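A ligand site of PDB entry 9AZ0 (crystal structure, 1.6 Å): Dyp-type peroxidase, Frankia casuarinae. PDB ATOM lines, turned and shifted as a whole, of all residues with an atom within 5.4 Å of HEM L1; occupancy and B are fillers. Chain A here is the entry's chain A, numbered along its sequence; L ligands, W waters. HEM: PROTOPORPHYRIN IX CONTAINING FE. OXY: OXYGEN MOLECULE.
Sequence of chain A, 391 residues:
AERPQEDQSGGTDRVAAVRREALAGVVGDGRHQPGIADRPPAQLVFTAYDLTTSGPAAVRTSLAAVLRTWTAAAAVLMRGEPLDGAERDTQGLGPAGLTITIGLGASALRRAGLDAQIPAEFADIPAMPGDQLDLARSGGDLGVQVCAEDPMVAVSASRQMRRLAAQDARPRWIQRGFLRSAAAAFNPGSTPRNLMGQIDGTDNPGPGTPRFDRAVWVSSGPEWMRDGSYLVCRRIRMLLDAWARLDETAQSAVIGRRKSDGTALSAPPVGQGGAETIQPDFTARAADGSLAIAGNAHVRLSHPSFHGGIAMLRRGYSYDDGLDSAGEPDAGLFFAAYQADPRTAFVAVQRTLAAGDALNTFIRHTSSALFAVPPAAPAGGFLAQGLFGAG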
ATOM      1  N   ASN A 194     -14.617  -8.860   4.609  1.00  0.00           N
ATOM      2  CA  ASN A 194     -14.182 -10.217   4.880  1.00  0.00           C
ATOM      3  C   ASN A 194     -15.360 -11.009   5.426  1.00  0.00           C
ATOM      4  O   ASN A 194     -16.484 -10.501   5.539  1.00  0.00           O
ATOM      5  CB  ASN A 194     -12.969 -10.257   5.819  1.00  0.00           C
ATOM      6  CG  ASN A 194     -13.254  -9.629   7.186  1.00  0.00           C
ATOM      7  OD1 ASN A 194     -14.380  -9.637   7.660  1.00  0.00           O
ATOM      8  ND2 ASN A 194     -12.206  -9.136   7.848  1.00  0.00           N
ATOM      9  N   MET A 196     -16.044 -11.927   8.304  1.00  0.00           N
ATOM     10  CA  MET A 196     -16.500 -11.447   9.587  1.00  0.00           C
ATOM     11  C   MET A 196     -17.366 -10.208   9.397  1.00  0.00           C
ATOM     12  O   MET A 196     -17.863  -9.648  10.367  1.00  0.00           O
ATOM     13  CB  MET A 196     -15.228 -11.189  10.400  1.00  0.00           C
ATOM     14  CG  MET A 196     -15.018 -12.219  11.453  1.00  0.00           C
ATOM     15  SD  MET A 196     -13.448 -11.920  12.271  1.00  0.00           S
ATOM     16  CE  MET A 196     -13.359 -13.363  13.320  1.00  0.00           C
ATOM     17  N   GLN A 198     -16.347  -7.368   8.169  1.00  0.00           N
ATOM     18  CA  GLN A 198     -15.568  -6.153   8.376  1.00  0.00           C
ATOM     19  C   GLN A 198     -15.021  -5.614   7.061  1.00  0.00           C
ATOM     20  O   GLN A 198     -14.610  -6.370   6.189  1.00  0.00           O
ATOM     21  CB  GLN A 198     -14.398  -6.418   9.323  1.00  0.00           C
ATOM     22  CG  GLN A 198     -14.825  -6.942  10.682  1.00  0.00           C
ATOM     23  CD  GLN A 198     -13.825  -7.911  11.291  1.00  0.00           C
ATOM     24  OE1 GLN A 198     -12.910  -8.382  10.609  1.00  0.00           O
ATOM     25  NE2 GLN A 198     -14.002  -8.229  12.565  1.00  0.00           N
ATOM     26  N   ILE A 199     -15.023  -4.281   6.930  1.00  0.00           N
ATOM     27  CA  ILE A 199     -14.229  -3.640   5.887  1.00  0.00           C
ATOM     28  C   ILE A 199     -12.764  -3.948   6.169  1.00  0.00           C
ATOM     29  O   ILE A 199     -12.273  -3.682   7.274  1.00  0.00           O
ATOM     30  CB  ILE A 199     -14.507  -2.133   5.856  1.00  0.00           C
ATOM     31  CG1 ILE A 199     -15.947  -1.858   5.470  1.00  0.00           C
ATOM     32  CG2 ILE A 199     -13.554  -1.456   4.880  1.00  0.00           C
ATOM     33  CD1 ILE A 199     -16.421  -0.465   5.811  1.00  0.00           C
ATOM     34  N   ASP A 200     -12.081  -4.525   5.188  1.00  0.00           N
ATOM     35  CA  ASP A 200     -10.739  -5.072   5.385  1.00  0.00           C
ATOM     36  C   ASP A 200      -9.769  -4.460   4.370  1.00  0.00           C
ATOM     37  O   ASP A 200      -9.724  -4.885   3.205  1.00  0.00           O
ATOM     38  CB  ASP A 200     -10.780  -6.597   5.283  1.00  0.00           C
ATOM     39  CG  ASP A 200      -9.586  -7.261   5.925  1.00  0.00           C
ATOM     40  OD1 ASP A 200      -8.484  -6.668   5.869  1.00  0.00           O
ATOM     41  OD2 ASP A 200      -9.737  -8.368   6.509  1.00  0.00           O
ATOM     42  N   GLY A 201      -8.980  -3.477   4.818  1.00  0.00           N
ATOM     43  CA  GLY A 201      -7.933  -2.881   3.977  1.00  0.00           C
ATOM     44  C   GLY A 201      -7.800  -1.371   4.083  1.00  0.00           C
ATOM     45  O   GLY A 201      -6.924  -0.792   3.438  1.00  0.00           O
ATOM     46  N   THR A 202      -8.644  -0.748   4.901  1.00  0.00           N
ATOM     47  CA  THR A 202      -8.766   0.715   4.957  1.00  0.00           C
ATOM     48  C   THR A 202      -7.411   1.389   5.145  1.00  0.00           C
ATOM     49  O   THR A 202      -7.077   2.349   4.438  1.00  0.00           O
ATOM     50  CB  THR A 202      -9.724   1.096   6.081  1.00  0.00           C
ATOM     51  OG1 THR A 202     -11.024   0.554   5.796  1.00  0.00           O
ATOM     52  CG2 THR A 202      -9.843   2.622   6.196  1.00  0.00           C
ATOM     53  N   ASP A 203      -6.615   0.939   6.113  1.00  0.00           N
ATOM     54  CA  ASP A 203      -5.376   1.641   6.425  1.00  0.00           C
ATOM     55  C   ASP A 203      -4.159   1.059   5.709  1.00  0.00           C
ATOM     56  O   ASP A 203      -3.021   1.417   6.060  1.00  0.00           O
ATOM     57  CB  ASP A 203      -5.156   1.688   7.941  1.00  0.00           C
ATOM     58  CG  ASP A 203      -5.899   2.863   8.610  1.00  0.00           C
ATOM     59  OD1 ASP A 203      -6.573   3.629   7.874  1.00  0.00           O
ATOM     60  OD2 ASP A 203      -5.803   3.046   9.855  1.00  0.00           O
ATOM     61  N   ASN A 204      -4.360   0.199   4.709  1.00  0.00           N
ATOM     62  CA  ASN A 204      -3.303  -0.135   3.778  1.00  0.00           C
ATOM     63  C   ASN A 204      -2.736   1.140   3.147  1.00  0.00           C
ATOM     64  O   ASN A 204      -3.487   2.076   2.859  1.00  0.00           O
ATOM     65  CB  ASN A 204      -3.836  -1.016   2.648  1.00  0.00           C
ATOM     66  CG  ASN A 204      -3.709  -2.471   2.917  1.00  0.00           C
ATOM     67  OD1 ASN A 204      -2.832  -2.920   3.646  1.00  0.00           O
ATOM     68  ND2 ASN A 204      -4.607  -3.251   2.307  1.00  0.00           N
ATOM     69  N   ARG A 211       4.423   6.370   0.539  1.00  0.00           N
ATOM     70  CA  ARG A 211       4.151   5.521   1.703  1.00  0.00           C
ATOM     71  C   ARG A 211       4.110   4.044   1.310  1.00  0.00           C
ATOM     72  O   ARG A 211       4.665   3.189   2.010  1.00  0.00           O
ATOM     73  CB  ARG A 211       2.849   5.958   2.382  1.00  0.00           C
ATOM     74  CG  ARG A 211       2.288   4.936   3.356  1.00  0.00           C
ATOM     75  CD  ARG A 211       1.021   5.428   4.069  1.00  0.00           C
ATOM     76  NE  ARG A 211       0.994   4.975   5.453  1.00  0.00           N
ATOM     77  CZ  ARG A 211       0.052   4.185   5.968  1.00  0.00           C
ATOM     78  NH1 ARG A 211      -0.977   3.789   5.249  1.00  0.00           N
ATOM     79  NH2 ARG A 211       0.170   3.785   7.230  1.00  0.00           N
ATOM     80  N   ILE A 236      -5.607 -18.115   8.171  1.00  0.00           N
ATOM     81  CA  ILE A 236      -6.186 -17.818   9.471  1.00  0.00           C
ATOM     82  C   ILE A 236      -7.647 -18.238   9.468  1.00  0.00           C
ATOM     83  O   ILE A 236      -8.492 -17.601   8.838  1.00  0.00           O
ATOM     84  CB  ILE A 236      -6.048 -16.340   9.836  1.00  0.00           C
ATOM     85  CG1 ILE A 236      -4.610 -15.865   9.637  1.00  0.00           C
ATOM     86  CG2 ILE A 236      -6.504 -16.102  11.286  1.00  0.00           C
ATOM     87  CD1 ILE A 236      -4.394 -14.328   9.918  1.00  0.00           C
ATOM     88  N   MET A 238     -11.350 -18.517  10.818  1.00  0.00           N
ATOM     89  CA  MET A 238     -12.253 -17.680  11.598  1.00  0.00           C
ATOM     90  C   MET A 238     -13.268 -18.571  12.306  1.00  0.00           C
ATOM     91  O   MET A 238     -13.867 -19.429  11.671  1.00  0.00           O
ATOM     92  CB  MET A 238     -12.978 -16.695  10.674  1.00  0.00           C
ATOM     93  CG  MET A 238     -12.153 -15.504  10.212  1.00  0.00           C
ATOM     94  SD  MET A 238     -13.007 -14.682   8.852  1.00  0.00           S
ATOM     95  CE  MET A 238     -12.061 -13.154   8.782  1.00  0.00           C
ATOM     96  N   ILE A 255     -12.331  -4.971  17.079  1.00  0.00           N
ATOM     97  CA  ILE A 255     -11.442  -4.383  16.073  1.00  0.00           C
ATOM     98  C   ILE A 255     -10.996  -2.988  16.482  1.00  0.00           C
ATOM     99  O   ILE A 255      -9.837  -2.610  16.250  1.00  0.00           O
ATOM    100  CB  ILE A 255     -12.156  -4.366  14.712  1.00  0.00           C
ATOM    101  CG1 ILE A 255     -12.347  -5.801  14.195  1.00  0.00           C
ATOM    102  CG2 ILE A 255     -11.412  -3.517  13.684  1.00  0.00           C
ATOM    103  CD1 ILE A 255     -11.041  -6.589  14.061  1.00  0.00           C
ATOM    104  N   ARG A 257     -13.107  -0.485  15.287  1.00  0.00           N
ATOM    105  CA  ARG A 257     -13.806   0.262  14.256  1.00  0.00           C
ATOM    106  C   ARG A 257     -15.242  -0.240  14.171  1.00  0.00           C
ATOM    107  O   ARG A 257     -15.504  -1.426  14.396  1.00  0.00           O
ATOM    108  CB  ARG A 257     -13.156   0.080  12.880  1.00  0.00           C
ATOM    109  CG  ARG A 257     -11.808   0.768  12.788  1.00  0.00           C
ATOM    110  CD  ARG A 257     -11.217   0.565  11.399  1.00  0.00           C
ATOM    111  NE  ARG A 257      -9.975   1.292  11.208  1.00  0.00           N
ATOM    112  CZ  ARG A 257      -9.887   2.536  10.774  1.00  0.00           C
ATOM    113  NH1 ARG A 257     -10.962   3.270  10.544  1.00  0.00           N
ATOM    114  NH2 ARG A 257      -8.682   3.072  10.581  1.00  0.00           N
ATOM    115  N   GLN A 279      -8.067   8.955  11.235  1.00  0.00           N
ATOM    116  CA  GLN A 279      -7.250   8.004  11.956  1.00  0.00           C
ATOM    117  C   GLN A 279      -7.781   7.741  13.372  1.00  0.00           C
ATOM    118  O   GLN A 279      -8.359   8.630  14.007  1.00  0.00           O
ATOM    119  CB  GLN A 279      -5.806   8.511  12.044  1.00  0.00           C
ATOM    120  CG  GLN A 279      -5.002   8.313  10.772  1.00  0.00           C
ATOM    121  CD  GLN A 279      -4.632   6.863  10.561  1.00  0.00           C
ATOM    122  OE1 GLN A 279      -4.093   6.227  11.458  1.00  0.00           O
ATOM    123  NE2 GLN A 279      -4.913   6.336   9.381  1.00  0.00           N
ATOM    124  N   PRO A 280      -7.573   6.528  13.884  1.00  0.00           N
ATOM    125  CA  PRO A 280      -7.921   6.256  15.282  1.00  0.00           C
ATOM    126  C   PRO A 280      -7.147   7.157  16.235  1.00  0.00           C
ATOM    127  O   PRO A 280      -6.011   7.546  15.977  1.00  0.00           O
ATOM    128  CB  PRO A 280      -7.527   4.789  15.455  1.00  0.00           C
ATOM    129  CG  PRO A 280      -6.515   4.523  14.397  1.00  0.00           C
ATOM    130  CD  PRO A 280      -6.897   5.387  13.239  1.00  0.00           C
ATOM    131  N   HIS A 298      -7.861  -4.772  18.001  1.00  0.00           N
ATOM    132  CA  HIS A 298      -6.977  -5.174  16.921  1.00  0.00           C
ATOM    133  C   HIS A 298      -6.259  -3.985  16.294  1.00  0.00           C
ATOM    134  O   HIS A 298      -5.038  -4.031  16.071  1.00  0.00           O
ATOM    135  CB  HIS A 298      -7.816  -5.914  15.865  1.00  0.00           C
ATOM    136  CG  HIS A 298      -7.027  -6.399  14.696  1.00  0.00           C
ATOM    137  ND1 HIS A 298      -6.160  -7.468  14.780  1.00  0.00           N
ATOM    138  CD2 HIS A 298      -6.983  -5.979  13.413  1.00  0.00           C
ATOM    139  CE1 HIS A 298      -5.617  -7.695  13.600  1.00  0.00           C
ATOM    140  NE2 HIS A 298      -6.092  -6.793  12.752  1.00  0.00           N
ATOM    141  N   VAL A 299      -6.993  -2.911  16.000  1.00  0.00           N
ATOM    142  CA  VAL A 299      -6.400  -1.759  15.321  1.00  0.00           C
ATOM    143  C   VAL A 299      -5.415  -1.037  16.232  1.00  0.00           C
ATOM    144  O   VAL A 299      -4.407  -0.494  15.762  1.00  0.00           O
ATOM    145  CB  VAL A 299      -7.511  -0.830  14.801  1.00  0.00           C
ATOM    146  CG1 VAL A 299      -6.964   0.545  14.404  1.00  0.00           C
ATOM    147  CG2 VAL A 299      -8.196  -1.490  13.619  1.00  0.00           C
ATOM    148  N   SER A 302      -2.110  -3.173  16.199  1.00  0.00           N
ATOM    149  CA  SER A 302      -1.440  -3.279  14.907  1.00  0.00           C
ATOM    150  C   SER A 302      -1.038  -1.933  14.295  1.00  0.00           C
ATOM    151  O   SER A 302      -0.341  -1.904  13.275  1.00  0.00           O
ATOM    152  CB  SER A 302      -2.352  -4.044  13.924  1.00  0.00           C
ATOM    153  OG  SER A 302      -3.507  -3.288  13.628  1.00  0.00           O
ATOM    154  N   HIS A 303      -1.426  -0.822  14.912  1.00  0.00           N
ATOM    155  CA  HIS A 303      -1.277   0.460  14.246  1.00  0.00           C
ATOM    156  C   HIS A 303       0.195   0.835  14.138  1.00  0.00           C
ATOM    157  O   HIS A 303       0.976   0.554  15.057  1.00  0.00           O
ATOM    158  CB  HIS A 303      -2.046   1.538  15.007  1.00  0.00           C
ATOM    159  CG  HIS A 303      -2.172   2.835  14.260  1.00  0.00           C
ATOM    160  ND1 HIS A 303      -1.271   3.863  14.392  1.00  0.00           N
ATOM    161  CD2 HIS A 303      -3.093   3.245  13.354  1.00  0.00           C
ATOM    162  CE1 HIS A 303      -1.631   4.858  13.603  1.00  0.00           C
ATOM    163  NE2 HIS A 303      -2.733   4.506  12.957  1.00  0.00           N
ATOM    164  N   PRO A 304       0.622   1.455  13.032  1.00  0.00           N
ATOM    165  CA  PRO A 304       2.048   1.804  12.866  1.00  0.00           C
ATOM    166  C   PRO A 304       2.615   2.639  14.005  1.00  0.00           C
ATOM    167  O   PRO A 304       3.817   2.535  14.286  1.00  0.00           O
ATOM    168  CB  PRO A 304       2.073   2.577  11.547  1.00  0.00           C
ATOM    169  CG  PRO A 304       0.907   2.013  10.770  1.00  0.00           C
ATOM    170  CD  PRO A 304      -0.156   1.767  11.818  1.00  0.00           C
ATOM    171  N   MET A 312       2.465  -2.043   6.334  1.00  0.00           N
ATOM    172  CA  MET A 312       2.521  -3.245   5.535  1.00  0.00           C
ATOM    173  C   MET A 312       1.354  -3.210   4.568  1.00  0.00           C
ATOM    174  O   MET A 312       0.369  -2.500   4.797  1.00  0.00           O
ATOM    175  CB  MET A 312       2.551  -4.465   6.458  1.00  0.00           C
ATOM    176  CG  MET A 312       1.177  -4.895   6.947  1.00  0.00           C
ATOM    177  SD  MET A 312       1.305  -6.294   8.067  1.00  0.00           S
ATOM    178  CE  MET A 312       2.020  -5.481   9.489  1.00  0.00           C
ATOM    179  N   ARG A 314      -1.509  -5.392   3.251  1.00  0.00           N
ATOM    180  CA  ARG A 314      -2.298  -6.601   3.457  1.00  0.00           C
ATOM    181  C   ARG A 314      -3.086  -6.854   2.181  1.00  0.00           C
ATOM    182  O   ARG A 314      -3.887  -6.014   1.765  1.00  0.00           O
ATOM    183  CB  ARG A 314      -3.226  -6.427   4.659  1.00  0.00           C
ATOM    184  CG  ARG A 314      -2.445  -6.503   5.980  1.00  0.00           C
ATOM    185  CD  ARG A 314      -3.260  -5.966   7.145  1.00  0.00           C
ATOM    186  NE  ARG A 314      -3.554  -4.545   6.983  1.00  0.00           N
ATOM    187  CZ  ARG A 314      -4.779  -4.053   6.943  1.00  0.00           C
ATOM    188  NH1 ARG A 314      -5.851  -4.817   7.104  1.00  0.00           N
ATOM    189  NH2 ARG A 314      -4.938  -2.738   6.767  1.00  0.00           N
ATOM    190  N   LEU A 333      -9.545 -16.231   6.571  1.00  0.00           N
ATOM    191  CA  LEU A 333      -8.789 -15.249   5.818  1.00  0.00           C
ATOM    192  C   LEU A 333      -7.433 -15.844   5.499  1.00  0.00           C
ATOM    193  O   LEU A 333      -6.679 -16.214   6.422  1.00  0.00           O
ATOM    194  CB  LEU A 333      -8.610 -13.948   6.625  1.00  0.00           C
ATOM    195  CG  LEU A 333      -7.754 -12.861   5.970  1.00  0.00           C
ATOM    196  CD1 LEU A 333      -8.521 -12.316   4.772  1.00  0.00           C
ATOM    197  CD2 LEU A 333      -7.475 -11.766   6.989  1.00  0.00           C
ATOM    198  N   PHE A 335      -4.365 -14.658   4.867  1.00  0.00           N
ATOM    199  CA  PHE A 335      -3.618 -13.433   5.069  1.00  0.00           C
ATOM    200  C   PHE A 335      -2.343 -13.454   4.218  1.00  0.00           C
ATOM    201  O   PHE A 335      -1.628 -14.456   4.194  1.00  0.00           O
ATOM    202  CB  PHE A 335      -3.301 -13.337   6.564  1.00  0.00           C
ATOM    203  CG  PHE A 335      -2.522 -12.104   6.960  1.00  0.00           C
ATOM    204  CD1 PHE A 335      -1.135 -12.077   6.864  1.00  0.00           C
ATOM    205  CD2 PHE A 335      -3.181 -11.000   7.467  1.00  0.00           C
ATOM    206  CE1 PHE A 335      -0.434 -10.948   7.252  1.00  0.00           C
ATOM    207  CE2 PHE A 335      -2.484  -9.864   7.849  1.00  0.00           C
ATOM    208  CZ  PHE A 335      -1.100  -9.838   7.737  1.00  0.00           C
ATOM    209  N   PHE A 346       5.347  -7.679   9.701  1.00  0.00           N
ATOM    210  CA  PHE A 346       4.521  -8.795  10.156  1.00  0.00           C
ATOM    211  C   PHE A 346       4.915  -9.286  11.536  1.00  0.00           C
ATOM    212  O   PHE A 346       4.070  -9.467  12.408  1.00  0.00           O
ATOM    213  CB  PHE A 346       4.597  -9.981   9.183  1.00  0.00           C
ATOM    214  CG  PHE A 346       3.830 -11.174   9.697  1.00  0.00           C
ATOM    215  CD1 PHE A 346       2.446 -11.201   9.626  1.00  0.00           C
ATOM    216  CD2 PHE A 346       4.485 -12.211  10.357  1.00  0.00           C
ATOM    217  CE1 PHE A 346       1.724 -12.270  10.153  1.00  0.00           C
ATOM    218  CE2 PHE A 346       3.772 -13.266  10.899  1.00  0.00           C
ATOM    219  CZ  PHE A 346       2.387 -13.290  10.797  1.00  0.00           C
ATOM    220  N   VAL A 349       4.301  -6.883  14.512  1.00  0.00           N
ATOM    221  CA  VAL A 349       2.879  -6.705  14.780  1.00  0.00           C
ATOM    222  C   VAL A 349       2.281  -7.981  15.340  1.00  0.00           C
ATOM    223  O   VAL A 349       1.544  -7.949  16.340  1.00  0.00           O
ATOM    224  CB  VAL A 349       2.150  -6.240  13.497  1.00  0.00           C
ATOM    225  CG1 VAL A 349       0.635  -6.195  13.728  1.00  0.00           C
ATOM    226  CG2 VAL A 349       2.681  -4.884  13.051  1.00  0.00           C
ATOM    227  N   GLN A 350       2.592  -9.141  14.734  1.00  0.00           N
ATOM    228  CA  GLN A 350       1.980 -10.383  15.211  1.00  0.00           C
ATOM    229  C   GLN A 350       2.409 -10.710  16.645  1.00  0.00           C
ATOM    230  O   GLN A 350       1.598 -11.218  17.429  1.00  0.00           O
ATOM    231  CB  GLN A 350       2.284 -11.533  14.255  1.00  0.00           C
ATOM    232  CG  GLN A 350       1.678 -12.880  14.699  1.00  0.00           C
ATOM    233  CD  GLN A 350       0.164 -12.823  14.828  1.00  0.00           C
ATOM    234  OE1 GLN A 350      -0.488 -12.019  14.178  1.00  0.00           O
ATOM    235  NE2 GLN A 350      -0.400 -13.712  15.652  1.00  0.00           N
ATOM    236  N   LEU A 353      -0.013  -8.776  18.642  1.00  0.00           N
ATOM    237  CA  LEU A 353      -1.355  -9.355  18.550  1.00  0.00           C
ATOM    238  C   LEU A 353      -1.459 -10.633  19.366  1.00  0.00           C
ATOM    239  O   LEU A 353      -2.457 -10.845  20.075  1.00  0.00           O
ATOM    240  CB  LEU A 353      -1.705  -9.652  17.088  1.00  0.00           C
ATOM    241  CG  LEU A 353      -1.738  -8.459  16.133  1.00  0.00           C
ATOM    242  CD1 LEU A 353      -2.226  -8.872  14.745  1.00  0.00           C
ATOM    243  CD2 LEU A 353      -2.596  -7.318  16.701  1.00  0.00           C
ATOM    244  N   LEU A 359      -9.168  -9.983  19.082  1.00  0.00           N
ATOM    245  CA  LEU A 359      -9.515 -10.835  17.948  1.00  0.00           C
ATOM    246  C   LEU A 359      -9.088 -12.276  18.152  1.00  0.00           C
ATOM    247  O   LEU A 359      -9.666 -13.163  17.522  1.00  0.00           O
ATOM    248  CB  LEU A 359      -8.877 -10.296  16.671  1.00  0.00           C
ATOM    249  CG  LEU A 359      -9.247 -10.941  15.338  1.00  0.00           C
ATOM    250  CD1 LEU A 359     -10.731 -10.801  15.088  1.00  0.00           C
ATOM    251  CD2 LEU A 359      -8.466 -10.242  14.256  1.00  0.00           C
ATOM    252  N   ILE A 363     -10.027 -16.363  16.051  1.00  0.00           N
ATOM    253  CA  ILE A 363      -9.192 -16.736  14.913  1.00  0.00           C
ATOM    254  C   ILE A 363      -8.161 -17.774  15.355  1.00  0.00           C
ATOM    255  O   ILE A 363      -7.806 -17.866  16.532  1.00  0.00           O
ATOM    256  CB  ILE A 363      -8.477 -15.528  14.261  1.00  0.00           C
ATOM    257  CG1 ILE A 363      -7.540 -14.837  15.257  1.00  0.00           C
ATOM    258  CG2 ILE A 363      -9.507 -14.537  13.728  1.00  0.00           C
ATOM    259  CD1 ILE A 363      -6.637 -13.850  14.589  1.00  0.00           C
ATOM    260  N   HIS A 365      -4.372 -19.213  13.667  1.00  0.00           N
ATOM    261  CA  HIS A 365      -3.393 -19.270  12.584  1.00  0.00           C
ATOM    262  C   HIS A 365      -3.031 -20.720  12.310  1.00  0.00           C
ATOM    263  O   HIS A 365      -2.428 -21.391  13.166  1.00  0.00           O
ATOM    264  CB  HIS A 365      -2.142 -18.480  12.951  1.00  0.00           C
ATOM    265  CG  HIS A 365      -2.357 -17.002  13.003  1.00  0.00           C
ATOM    266  ND1 HIS A 365      -1.622 -16.121  12.236  1.00  0.00           N
ATOM    267  CD2 HIS A 365      -3.203 -16.242  13.742  1.00  0.00           C
ATOM    268  CE1 HIS A 365      -2.020 -14.888  12.492  1.00  0.00           C
ATOM    269  NE2 HIS A 365      -2.978 -14.935  13.401  1.00  0.00           N
HETATM  270  CHA HEM L   1      -6.372  -3.608  10.271  1.00  0.00           C
HETATM  271  CHB HEM L   1      -9.155  -7.617  10.384  1.00  0.00           C
HETATM  272  CHC HEM L   1      -5.175 -10.393  10.860  1.00  0.00           C
HETATM  273  CHD HEM L   1      -2.414  -6.404  10.766  1.00  0.00           C
HETATM  274  C1A HEM L   1      -7.461  -4.455  10.272  1.00  0.00           C
HETATM  275  C2A HEM L   1      -8.848  -4.050  10.170  1.00  0.00           C
HETATM  276  C3A HEM L   1      -9.604  -5.156  10.203  1.00  0.00           C
HETATM  277  C4A HEM L   1      -8.735  -6.302  10.324  1.00  0.00           C
HETATM  278  CMA HEM L   1     -11.148  -5.229  10.137  1.00  0.00           C
HETATM  279  CAA HEM L   1      -9.374  -2.585  10.094  1.00  0.00           C
HETATM  280  CBA HEM L   1      -9.508  -2.008   8.693  1.00  0.00           C
HETATM  281  CGA HEM L   1      -8.177  -1.864   7.986  1.00  0.00           C
HETATM  282  O1A HEM L   1      -7.440  -0.880   8.261  1.00  0.00           O
HETATM  283  O2A HEM L   1      -7.864  -2.736   7.137  1.00  0.00           O
HETATM  284  C1B HEM L   1      -8.304  -8.698  10.544  1.00  0.00           C
HETATM  285  C2B HEM L   1      -8.728 -10.075  10.628  1.00  0.00           C
HETATM  286  C3B HEM L   1      -7.642 -10.857  10.777  1.00  0.00           C
HETATM  287  C4B HEM L   1      -6.485  -9.976  10.751  1.00  0.00           C
HETATM  288  CMB HEM L   1     -10.212 -10.463  10.591  1.00  0.00           C
HETATM  289  CAB HEM L   1      -7.572 -12.402  10.894  1.00  0.00           C
HETATM  290  CBB HEM L   1      -8.499 -13.171  10.297  1.00  0.00           C
HETATM  291  C1C HEM L   1      -4.073  -9.558  10.905  1.00  0.00           C
HETATM  292  C2C HEM L   1      -2.690  -9.956  11.084  1.00  0.00           C
HETATM  293  C3C HEM L   1      -1.931  -8.845  11.038  1.00  0.00           C
HETATM  294  C4C HEM L   1      -2.812  -7.713  10.856  1.00  0.00           C
HETATM  295  CMC HEM L   1      -2.244 -11.441  11.240  1.00  0.00           C
HETATM  296  CAC HEM L   1      -0.393  -8.665  11.190  1.00  0.00           C
HETATM  297  CBC HEM L   1       0.357  -9.513  11.904  1.00  0.00           C
HETATM  298  C1D HEM L   1      -3.234  -5.311  10.556  1.00  0.00           C
HETATM  299  C2D HEM L   1      -2.790  -3.967  10.322  1.00  0.00           C
HETATM  300  C3D HEM L   1      -3.872  -3.183  10.190  1.00  0.00           C
HETATM  301  C4D HEM L   1      -5.054  -4.021  10.330  1.00  0.00           C
HETATM  302  CMD HEM L   1      -1.316  -3.537  10.232  1.00  0.00           C
HETATM  303  CAD HEM L   1      -3.891  -1.673   9.921  1.00  0.00           C
HETATM  304  CBD HEM L   1      -3.586  -0.902  11.209  1.00  0.00           C
HETATM  305  CGD HEM L   1      -3.746   0.562  10.935  1.00  0.00           C
HETATM  306  O1D HEM L   1      -2.823   1.178  10.329  1.00  0.00           O
HETATM  307  O2D HEM L   1      -4.819   1.127  11.294  1.00  0.00           O
HETATM  308  NA  HEM L   1      -7.418  -5.849  10.340  1.00  0.00           N
HETATM  309  NB  HEM L   1      -6.931  -8.678  10.595  1.00  0.00           N
HETATM  310  NC  HEM L   1      -4.115  -8.175  10.772  1.00  0.00           N
HETATM  311  ND  HEM L   1      -4.632  -5.320  10.563  1.00  0.00           N
HETATM  312 FE   HEM L   1      -5.803  -6.963  10.685  1.00  0.00          FE
HETATM  313  O1  OXY L   2      -6.268  -8.102   6.922  1.00  0.00           O
HETATM  314  O2  OXY L   2      -6.007  -7.641   8.031  1.00  0.00           O
HETATM  315  O   HOH W   1       1.312  -1.533  10.644  1.00  0.00           O
HETATM  316  O   HOH W   2     -12.920  -2.015   9.372  1.00  0.00           O
HETATM  317  O   HOH W   3      -1.204   1.111   8.023  1.00  0.00           O
HETATM  318  O   HOH W   4      -7.308   0.265  10.695  1.00  0.00           O
HETATM  319  O   HOH W   5       0.163  -1.268   8.204  1.00  0.00           O
HETATM  320  O   HOH W   6      -2.628   3.938   9.721  1.00  0.00           O
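A ring nitrogen (NE2) of His 298 binds an iron atom (FE) of HEM L1 (2.1 Å).
The backbone NH of Asp 203 is in hydrogen-bond range of an oxygen (O1A) of HEM L1 (2.9 Å).
An oxygen (O2D) of HEM L1 sits close to the side-chain carboxylate (OD2) of Asp 203 (2.6 Å).
The backbone NH of Gly 201 sits at hydrogen-bond distance from an oxygen (O2A) of HEM L1, at 2.7 Å.
The guanidinium group (NH1) of Arg 314 lies within salt-bridge range of an oxygen (O2A) of HEM L1, at 2.9 Å.
The backbone NH (N) of Thr 202 is in hydrogen-bond range of an oxygen (O2A) of HEM L1 (3.1 Å).
O2 of OXY L2 is in hydrogen-bond range of NH1 of Arg 314 (3.0 Å).
Water W4 lies within hydrogen-bond range of an oxygen (O1A) of HEM L1 (2.7 Å), the guanidinium group of Arg 257 (2.9 Å) and the side-chain carboxylate of Asp 203 (3.3 Å).
Water W3 lies within hydrogen-bond range of O of Asp 203 (2.7 Å), O1D of HEM L1 (2.8 Å) and NH2 of Arg 211 (3.1 Å).
Water W6 lies within hydrogen-bond range of O1D of HEM L1 (2.8 Å), OE1 of Gln 279 (3.2 Å), NE2 of His 303 (3.3 Å) and OD2 of Asp 203 (3.3 Å).
Merely in contact with HEM L1: Pro 304, Phe 335, Ser 302, Gln 198, His 303, Ile 199, Gln 350, Phe 346, Leu 359, Asn 194, His 365, Ile 236, Val 349, Leu 353, Met 238, Leu 333, Asp 200, Val 299, Ile 363, Arg 257, Met 196, Met 312 and Ile 255.
Hydrophobic or aromatic side chains that line HEM L1: Met 196, Ile 236, Met 238, Ile 255, His 298, Val 299, His 303, Pro 304, Met 312, Leu 333, Phe 335, Phe 346, Val 349, Leu 353, Leu 359, Ile 363 and His 365.
The side-chain carboxylate of Asp 203 lies within salt-bridge range of the guanidinium group of Arg 257, 3.0 Å away.
The backbone carbonyl oxygen (O) of Asp 203 lies within hydrogen-bond range of the guanidinium group (NH1) of Arg 211, 3.2 Å away.
The side-chain carboxylate (OD2) of Asp 203 lies within hydrogen-bond range of the side-chain amide nitrogen (NE2) of Gln 279 (3.4 Å).
ND2 of Asn 194 sits at hydrogen-bond distance from OE1 of Gln 198 (2.9 Å).
NE2 of Gln 198 lies within hydrogen-bond range of SD of Met 196 (3.7 Å).
A ring nitrogen (NE2) of His 303 sits at hydrogen-bond distance from the side-chain amide oxygen (OE1) of Gln 279, at 2.7 Å.
The backbone NH (N) of Met 196 lies within hydrogen-bond range of the side-chain amide oxygen (OD1) of Asn 194 (2.9 Å).
The backbone NH (N) of Ile 236 lies within hydrogen-bond range of the backbone carbonyl oxygen (O) of Leu 333 (2.8 Å).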
